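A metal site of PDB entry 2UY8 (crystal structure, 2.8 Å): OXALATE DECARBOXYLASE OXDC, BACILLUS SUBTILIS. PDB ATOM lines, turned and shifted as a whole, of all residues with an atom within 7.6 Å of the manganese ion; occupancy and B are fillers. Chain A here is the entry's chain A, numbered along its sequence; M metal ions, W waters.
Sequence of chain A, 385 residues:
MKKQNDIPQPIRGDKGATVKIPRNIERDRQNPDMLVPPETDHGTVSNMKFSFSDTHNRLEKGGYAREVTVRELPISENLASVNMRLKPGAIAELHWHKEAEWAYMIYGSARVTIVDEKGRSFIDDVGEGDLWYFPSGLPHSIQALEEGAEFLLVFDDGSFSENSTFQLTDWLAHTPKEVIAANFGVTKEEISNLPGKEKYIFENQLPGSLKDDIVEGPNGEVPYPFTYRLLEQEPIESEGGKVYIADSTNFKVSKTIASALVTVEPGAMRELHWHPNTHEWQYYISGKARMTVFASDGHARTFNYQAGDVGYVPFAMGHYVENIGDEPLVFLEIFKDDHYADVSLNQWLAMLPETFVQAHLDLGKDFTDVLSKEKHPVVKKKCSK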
ATOM      1  N   VAL A 262      21.495  -5.627  19.598  1.00  0.00           N
ATOM      2  CA  VAL A 262      21.306  -5.253  18.221  1.00  0.00           C
ATOM      3  C   VAL A 262      20.057  -4.367  18.067  1.00  0.00           C
ATOM      4  O   VAL A 262      18.956  -4.671  18.591  1.00  0.00           O
ATOM      5  CB  VAL A 262      21.191  -6.502  17.300  1.00  0.00           C
ATOM      6  CG1 VAL A 262      20.816  -6.097  15.819  1.00  0.00           C
ATOM      7  CG2 VAL A 262      22.460  -7.333  17.360  1.00  0.00           C
ATOM      8  N   ARG A 270      19.067  -7.325  10.265  1.00  0.00           N
ATOM      9  CA  ARG A 270      20.335  -7.952  10.560  1.00  0.00           C
ATOM     10  C   ARG A 270      20.643  -8.839   9.329  1.00  0.00           C
ATOM     11  O   ARG A 270      19.829  -9.732   8.946  1.00  0.00           O
ATOM     12  CB  ARG A 270      20.176  -8.774  11.847  1.00  0.00           C
ATOM     13  CG  ARG A 270      21.436  -9.472  12.309  1.00  0.00           C
ATOM     14  CD  ARG A 270      22.360  -8.612  13.151  1.00  0.00           C
ATOM     15  NE  ARG A 270      23.550  -9.392  13.430  1.00  0.00           N
ATOM     16  CZ  ARG A 270      24.574  -9.502  12.582  1.00  0.00           C
ATOM     17  NH1 ARG A 270      24.574  -8.836  11.432  1.00  0.00           N
ATOM     18  NH2 ARG A 270      25.591 -10.284  12.883  1.00  0.00           N
ATOM     19  N   GLU A 271      21.782  -8.590   8.693  1.00  0.00           N
ATOM     20  CA  GLU A 271      22.089  -9.204   7.408  1.00  0.00           C
ATOM     21  C   GLU A 271      22.139 -10.729   7.488  1.00  0.00           C
ATOM     22  O   GLU A 271      22.244 -11.285   8.579  1.00  0.00           O
ATOM     23  CB  GLU A 271      23.393  -8.647   6.834  1.00  0.00           C
ATOM     24  CG  GLU A 271      24.624  -9.039   7.618  1.00  0.00           C
ATOM     25  CD  GLU A 271      25.935  -8.679   6.901  1.00  0.00           C
ATOM     26  OE1 GLU A 271      25.888  -8.481   5.636  1.00  0.00           O
ATOM     27  OE2 GLU A 271      27.007  -8.592   7.605  1.00  0.00           O
ATOM     28  N   HIS A 273      23.927 -13.965   7.627  1.00  0.00           N
ATOM     29  CA  HIS A 273      25.222 -14.333   8.234  1.00  0.00           C
ATOM     30  C   HIS A 273      25.096 -15.667   8.945  1.00  0.00           C
ATOM     31  O   HIS A 273      24.025 -16.271   8.953  1.00  0.00           O
ATOM     32  CB  HIS A 273      25.719 -13.272   9.224  1.00  0.00           C
ATOM     33  CG  HIS A 273      24.863 -13.136  10.432  1.00  0.00           C
ATOM     34  ND1 HIS A 273      23.657 -12.482  10.424  1.00  0.00           N
ATOM     35  CD2 HIS A 273      25.040 -13.568  11.701  1.00  0.00           C
ATOM     36  CE1 HIS A 273      23.119 -12.536  11.623  1.00  0.00           C
ATOM     37  NE2 HIS A 273      23.930 -13.194  12.416  1.00  0.00           N
ATOM     38  N   TRP A 274      26.208 -16.143   9.492  1.00  0.00           N
ATOM     39  CA  TRP A 274      26.197 -17.253  10.417  1.00  0.00           C
ATOM     40  C   TRP A 274      27.318 -17.067  11.421  1.00  0.00           C
ATOM     41  O   TRP A 274      28.129 -16.139  11.276  1.00  0.00           O
ATOM     42  CB  TRP A 274      26.331 -18.592   9.713  1.00  0.00           C
ATOM     43  CG  TRP A 274      27.718 -18.937   9.197  1.00  0.00           C
ATOM     44  CD1 TRP A 274      28.656 -19.672   9.839  1.00  0.00           C
ATOM     45  CD2 TRP A 274      28.265 -18.636   7.897  1.00  0.00           C
ATOM     46  NE1 TRP A 274      29.765 -19.833   9.035  1.00  0.00           N
ATOM     47  CE2 TRP A 274      29.547 -19.208   7.835  1.00  0.00           C
ATOM     48  CE3 TRP A 274      27.793 -17.925   6.783  1.00  0.00           C
ATOM     49  CZ2 TRP A 274      30.371 -19.100   6.713  1.00  0.00           C
ATOM     50  CZ3 TRP A 274      28.607 -17.808   5.680  1.00  0.00           C
ATOM     51  CH2 TRP A 274      29.886 -18.392   5.648  1.00  0.00           C
ATOM     52  N   HIS A 275      27.352 -17.945  12.432  1.00  0.00           N
ATOM     53  CA  HIS A 275      28.357 -17.884  13.465  1.00  0.00           C
ATOM     54  C   HIS A 275      29.236 -19.115  13.397  1.00  0.00           C
ATOM     55  O   HIS A 275      28.758 -20.234  13.535  1.00  0.00           O
ATOM     56  CB  HIS A 275      27.684 -17.747  14.814  1.00  0.00           C
ATOM     57  CG  HIS A 275      26.838 -16.525  14.896  1.00  0.00           C
ATOM     58  ND1 HIS A 275      27.390 -15.255  14.924  1.00  0.00           N
ATOM     59  CD2 HIS A 275      25.501 -16.354  14.887  1.00  0.00           C
ATOM     60  CE1 HIS A 275      26.421 -14.356  14.951  1.00  0.00           C
ATOM     61  NE2 HIS A 275      25.266 -15.000  14.923  1.00  0.00           N
ATOM     62  N   GLU A 280      23.724 -19.601  18.698  1.00  0.00           N
ATOM     63  CA  GLU A 280      23.134 -18.330  19.127  1.00  0.00           C
ATOM     64  C   GLU A 280      21.822 -18.496  19.878  1.00  0.00           C
ATOM     65  O   GLU A 280      20.917 -19.210  19.439  1.00  0.00           O
ATOM     66  CB  GLU A 280      22.886 -17.403  17.947  1.00  0.00           C
ATOM     67  CG  GLU A 280      22.158 -16.141  18.332  1.00  0.00           C
ATOM     68  CD  GLU A 280      22.053 -15.120  17.189  1.00  0.00           C
ATOM     69  OE1 GLU A 280      22.845 -15.221  16.194  1.00  0.00           O
ATOM     70  OE2 GLU A 280      21.174 -14.205  17.305  1.00  0.00           O
ATOM     71  N   GLN A 282      18.791 -16.013  21.509  1.00  0.00           N
ATOM     72  CA  GLN A 282      18.198 -14.673  21.295  1.00  0.00           C
ATOM     73  C   GLN A 282      17.153 -14.292  22.329  1.00  0.00           C
ATOM     74  O   GLN A 282      16.365 -15.120  22.751  1.00  0.00           O
ATOM     75  CB  GLN A 282      17.516 -14.604  19.922  1.00  0.00           C
ATOM     76  CG  GLN A 282      18.308 -15.193  18.778  1.00  0.00           C
ATOM     77  CD  GLN A 282      17.644 -14.980  17.435  1.00  0.00           C
ATOM     78  OE1 GLN A 282      16.415 -15.045  17.307  1.00  0.00           O
ATOM     79  NE2 GLN A 282      18.463 -14.736  16.412  1.00  0.00           N
ATOM     80  N   MET A 291      12.729 -14.415  11.246  1.00  0.00           N
ATOM     81  CA  MET A 291      14.045 -14.940  10.911  1.00  0.00           C
ATOM     82  C   MET A 291      13.903 -16.271  10.185  1.00  0.00           C
ATOM     83  O   MET A 291      13.042 -17.059  10.525  1.00  0.00           O
ATOM     84  CB  MET A 291      14.852 -15.161  12.179  1.00  0.00           C
ATOM     85  CG  MET A 291      16.150 -15.910  11.963  1.00  0.00           C
ATOM     86  SD  MET A 291      17.070 -16.130  13.496  1.00  0.00           S
ATOM     87  CE  MET A 291      15.986 -17.242  14.396  1.00  0.00           C
ATOM     88  N   VAL A 313      19.500 -20.002  17.255  1.00  0.00           N
ATOM     89  CA  VAL A 313      20.040 -20.458  15.991  1.00  0.00           C
ATOM     90  C   VAL A 313      21.171 -21.426  16.270  1.00  0.00           C
ATOM     91  O   VAL A 313      22.229 -20.973  16.759  1.00  0.00           O
ATOM     92  CB  VAL A 313      20.542 -19.269  15.172  1.00  0.00           C
ATOM     93  CG1 VAL A 313      21.303 -19.731  13.902  1.00  0.00           C
ATOM     94  CG2 VAL A 313      19.378 -18.380  14.765  1.00  0.00           C
ATOM     95  N   MET A 317      24.287 -22.478  11.441  1.00  0.00           N
ATOM     96  CA  MET A 317      23.137 -22.309  10.594  1.00  0.00           C
ATOM     97  C   MET A 317      23.035 -20.877  10.052  1.00  0.00           C
ATOM     98  O   MET A 317      23.243 -19.905  10.786  1.00  0.00           O
ATOM     99  CB  MET A 317      21.898 -22.705  11.363  1.00  0.00           C
ATOM    100  CG  MET A 317      21.865 -24.187  11.562  1.00  0.00           C
ATOM    101  SD  MET A 317      20.330 -24.862  12.172  1.00  0.00           S
ATOM    102  CE  MET A 317      20.718 -26.593  12.065  1.00  0.00           C
ATOM    103  N   HIS A 319      21.346 -17.462   8.868  1.00  0.00           N
ATOM    104  CA  HIS A 319      20.168 -16.672   9.236  1.00  0.00           C
ATOM    105  C   HIS A 319      20.261 -15.180   8.952  1.00  0.00           C
ATOM    106  O   HIS A 319      21.307 -14.658   8.625  1.00  0.00           O
ATOM    107  CB  HIS A 319      19.833 -16.871  10.722  1.00  0.00           C
ATOM    108  CG  HIS A 319      20.963 -16.542  11.653  1.00  0.00           C
ATOM    109  ND1 HIS A 319      22.115 -17.302  11.715  1.00  0.00           N
ATOM    110  CD2 HIS A 319      21.101 -15.558  12.570  1.00  0.00           C
ATOM    111  CE1 HIS A 319      22.930 -16.771  12.615  1.00  0.00           C
ATOM    112  NE2 HIS A 319      22.331 -15.718  13.153  1.00  0.00           N
ATOM    113  N   TYR A 320      19.103 -14.539   9.082  1.00  0.00           N
ATOM    114  CA  TYR A 320      18.965 -13.098   9.050  1.00  0.00           C
ATOM    115  C   TYR A 320      17.849 -12.756  10.060  1.00  0.00           C
ATOM    116  O   TYR A 320      17.121 -13.637  10.493  1.00  0.00           O
ATOM    117  CB  TYR A 320      18.567 -12.641   7.664  1.00  0.00           C
ATOM    118  CG  TYR A 320      17.194 -13.033   7.347  1.00  0.00           C
ATOM    119  CD1 TYR A 320      16.128 -12.169   7.579  1.00  0.00           C
ATOM    120  CD2 TYR A 320      16.913 -14.321   6.866  1.00  0.00           C
ATOM    121  CE1 TYR A 320      14.785 -12.580   7.308  1.00  0.00           C
ATOM    122  CE2 TYR A 320      15.591 -14.742   6.588  1.00  0.00           C
ATOM    123  CZ  TYR A 320      14.555 -13.851   6.820  1.00  0.00           C
ATOM    124  OH  TYR A 320      13.294 -14.248   6.516  1.00  0.00           O
ATOM    125  N   VAL A 321      17.739 -11.509  10.452  1.00  0.00           N
ATOM    126  CA  VAL A 321      16.642 -11.110  11.317  1.00  0.00           C
ATOM    127  C   VAL A 321      16.172  -9.776  10.774  1.00  0.00           C
ATOM    128  O   VAL A 321      16.910  -8.758  10.814  1.00  0.00           O
ATOM    129  CB  VAL A 321      17.051 -10.954  12.812  1.00  0.00           C
ATOM    130  CG1 VAL A 321      15.838 -10.693  13.636  1.00  0.00           C
ATOM    131  CG2 VAL A 321      17.712 -12.186  13.347  1.00  0.00           C
ATOM    132  N   PHE A 331      16.995  -6.586  19.901  1.00  0.00           N
ATOM    133  CA  PHE A 331      17.218  -7.943  20.409  1.00  0.00           C
ATOM    134  C   PHE A 331      18.646  -8.184  20.848  1.00  0.00           C
ATOM    135  O   PHE A 331      19.573  -7.468  20.461  1.00  0.00           O
ATOM    136  CB  PHE A 331      16.711  -9.023  19.440  1.00  0.00           C
ATOM    137  CG  PHE A 331      17.499  -9.126  18.161  1.00  0.00           C
ATOM    138  CD1 PHE A 331      18.493 -10.078  18.021  1.00  0.00           C
ATOM    139  CD2 PHE A 331      17.206  -8.316  17.078  1.00  0.00           C
ATOM    140  CE1 PHE A 331      19.200 -10.183  16.824  1.00  0.00           C
ATOM    141  CE2 PHE A 331      17.926  -8.406  15.902  1.00  0.00           C
ATOM    142  CZ  PHE A 331      18.913  -9.336  15.769  1.00  0.00           C
ATOM    143  N   GLU A 333      21.778 -11.002  21.075  1.00  0.00           N
ATOM    144  CA  GLU A 333      22.353 -12.239  20.541  1.00  0.00           C
ATOM    145  C   GLU A 333      23.289 -12.747  21.617  1.00  0.00           C
ATOM    146  O   GLU A 333      24.114 -11.974  22.102  1.00  0.00           O
ATOM    147  CB  GLU A 333      23.159 -11.972  19.272  1.00  0.00           C
ATOM    148  CG  GLU A 333      22.441 -11.242  18.129  1.00  0.00           C
ATOM    149  CD  GLU A 333      23.348 -11.061  16.929  1.00  0.00           C
ATOM    150  OE1 GLU A 333      24.546 -10.815  17.159  1.00  0.00           O
ATOM    151  OE2 GLU A 333      22.897 -11.165  15.769  1.00  0.00           O
ATOM    152  N   ILE A 334      23.152 -14.013  22.017  1.00  0.00           N
ATOM    153  CA  ILE A 334      23.925 -14.535  23.137  1.00  0.00           C
ATOM    154  C   ILE A 334      24.623 -15.822  22.691  1.00  0.00           C
ATOM    155  O   ILE A 334      23.987 -16.664  22.020  1.00  0.00           O
ATOM    156  CB  ILE A 334      22.996 -14.784  24.371  1.00  0.00           C
ATOM    157  CG1 ILE A 334      22.329 -13.471  24.808  1.00  0.00           C
ATOM    158  CG2 ILE A 334      23.747 -15.477  25.554  1.00  0.00           C
ATOM    159  CD1 ILE A 334      23.236 -12.482  25.475  1.00  0.00           C
ATOM    160  N   PHE A 335      25.906 -15.974  23.066  1.00  0.00           N
ATOM    161  CA  PHE A 335      26.788 -17.077  22.654  1.00  0.00           C
ATOM    162  C   PHE A 335      27.566 -17.593  23.855  1.00  0.00           C
ATOM    163  O   PHE A 335      28.164 -16.815  24.588  1.00  0.00           O
ATOM    164  CB  PHE A 335      27.768 -16.577  21.575  1.00  0.00           C
ATOM    165  CG  PHE A 335      27.077 -15.918  20.361  1.00  0.00           C
ATOM    166  CD1 PHE A 335      26.692 -16.682  19.266  1.00  0.00           C
ATOM    167  CD2 PHE A 335      26.760 -14.549  20.367  1.00  0.00           C
ATOM    168  CE1 PHE A 335      26.021 -16.111  18.204  1.00  0.00           C
ATOM    169  CE2 PHE A 335      26.076 -13.963  19.301  1.00  0.00           C
ATOM    170  CZ  PHE A 335      25.719 -14.742  18.211  1.00  0.00           C
ATOM    171  N   TYR A 340      32.716 -13.159  20.487  1.00  0.00           N
ATOM    172  CA  TYR A 340      31.762 -12.947  19.435  1.00  0.00           C
ATOM    173  C   TYR A 340      32.454 -13.179  18.067  1.00  0.00           C
ATOM    174  O   TYR A 340      33.630 -12.836  17.902  1.00  0.00           O
ATOM    175  CB  TYR A 340      31.189 -11.519  19.529  1.00  0.00           C
ATOM    176  CG  TYR A 340      30.101 -11.309  18.534  1.00  0.00           C
ATOM    177  CD1 TYR A 340      28.771 -11.427  18.904  1.00  0.00           C
ATOM    178  CD2 TYR A 340      30.402 -11.062  17.181  1.00  0.00           C
ATOM    179  CE1 TYR A 340      27.758 -11.273  17.973  1.00  0.00           C
ATOM    180  CE2 TYR A 340      29.397 -10.916  16.241  1.00  0.00           C
ATOM    181  CZ  TYR A 340      28.077 -11.017  16.652  1.00  0.00           C
ATOM    182  OH  TYR A 340      27.082 -10.868  15.753  1.00  0.00           O
ATOM    183  N   ALA A 341      31.736 -13.756  17.101  1.00  0.00           N
ATOM    184  CA  ALA A 341      32.271 -13.949  15.752  1.00  0.00           C
ATOM    185  C   ALA A 341      31.142 -14.188  14.793  1.00  0.00           C
ATOM    186  O   ALA A 341      30.199 -14.944  15.111  1.00  0.00           O
ATOM    187  CB  ALA A 341      33.223 -15.126  15.698  1.00  0.00           C
ATOM    188  N   ASP A 342      31.221 -13.579  13.616  1.00  0.00           N
ATOM    189  CA  ASP A 342      30.267 -13.892  12.581  1.00  0.00           C
ATOM    190  C   ASP A 342      30.956 -13.866  11.230  1.00  0.00           C
ATOM    191  O   ASP A 342      32.070 -13.381  11.106  1.00  0.00           O
ATOM    192  CB  ASP A 342      29.003 -12.995  12.626  1.00  0.00           C
ATOM    193  CG  ASP A 342      29.299 -11.491  12.383  1.00  0.00           C
ATOM    194  OD1 ASP A 342      30.476 -11.102  12.164  1.00  0.00           O
ATOM    195  OD2 ASP A 342      28.361 -10.672  12.411  1.00  0.00           O
HETATM  196 MN    MN M   1      23.391 -14.201  14.466  1.00  0.00          MN
HETATM  197  O   HOH W   1      21.741 -12.863  14.592  1.00  0.00           O
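O of Ala 341 sits at hydrogen-bond distance from ND1 of His 275. The side-chain carboxylate (OE2) of Glu 280 lies within hydrogen-bond range of the side-chain amide nitrogen (NE2) of Gln 282, at 2.9 Å. The guanidinium group (NE) of Arg 270 is in salt-bridge range of the side-chain carboxylate (OE2) of Glu 333. The side-chain carboxylate (OE1) of Glu 333 is in hydrogen-bond range of the side-chain hydroxyl (OH) of Tyr 340 (2.9 Å). O of Glu 280 is in hydrogen-bond range of N of Val 313, at 2.7 Å. ND1 of His 273 sits at hydrogen-bond distance from O of Glu 271 (2.6 Å). NE2 of His 273 lies close to NH2 of Arg 270 (3.4 Å). The backbone carbonyl oxygen (O) of Met 317 sits at hydrogen-bond distance from a ring nitrogen (ND1) of His 319.
Merely in contact with the manganese ion: Glu 333. Along chain A the residues within 4 Å of the manganese ion span positions 273 to 333.
OE1 of Glu 280 binds the manganese ion (2.1 Å). NE2 of His 275 binds the manganese ion, 2.1 Å away. The manganese ion is bound by water W1 (2.1 Å). The manganese ion is bound by NE2 of His 319 (2.3 Å). NE2 of His 273 is bound to the manganese ion (2.3 Å). The manganese ion has five donor atoms within binding distance.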
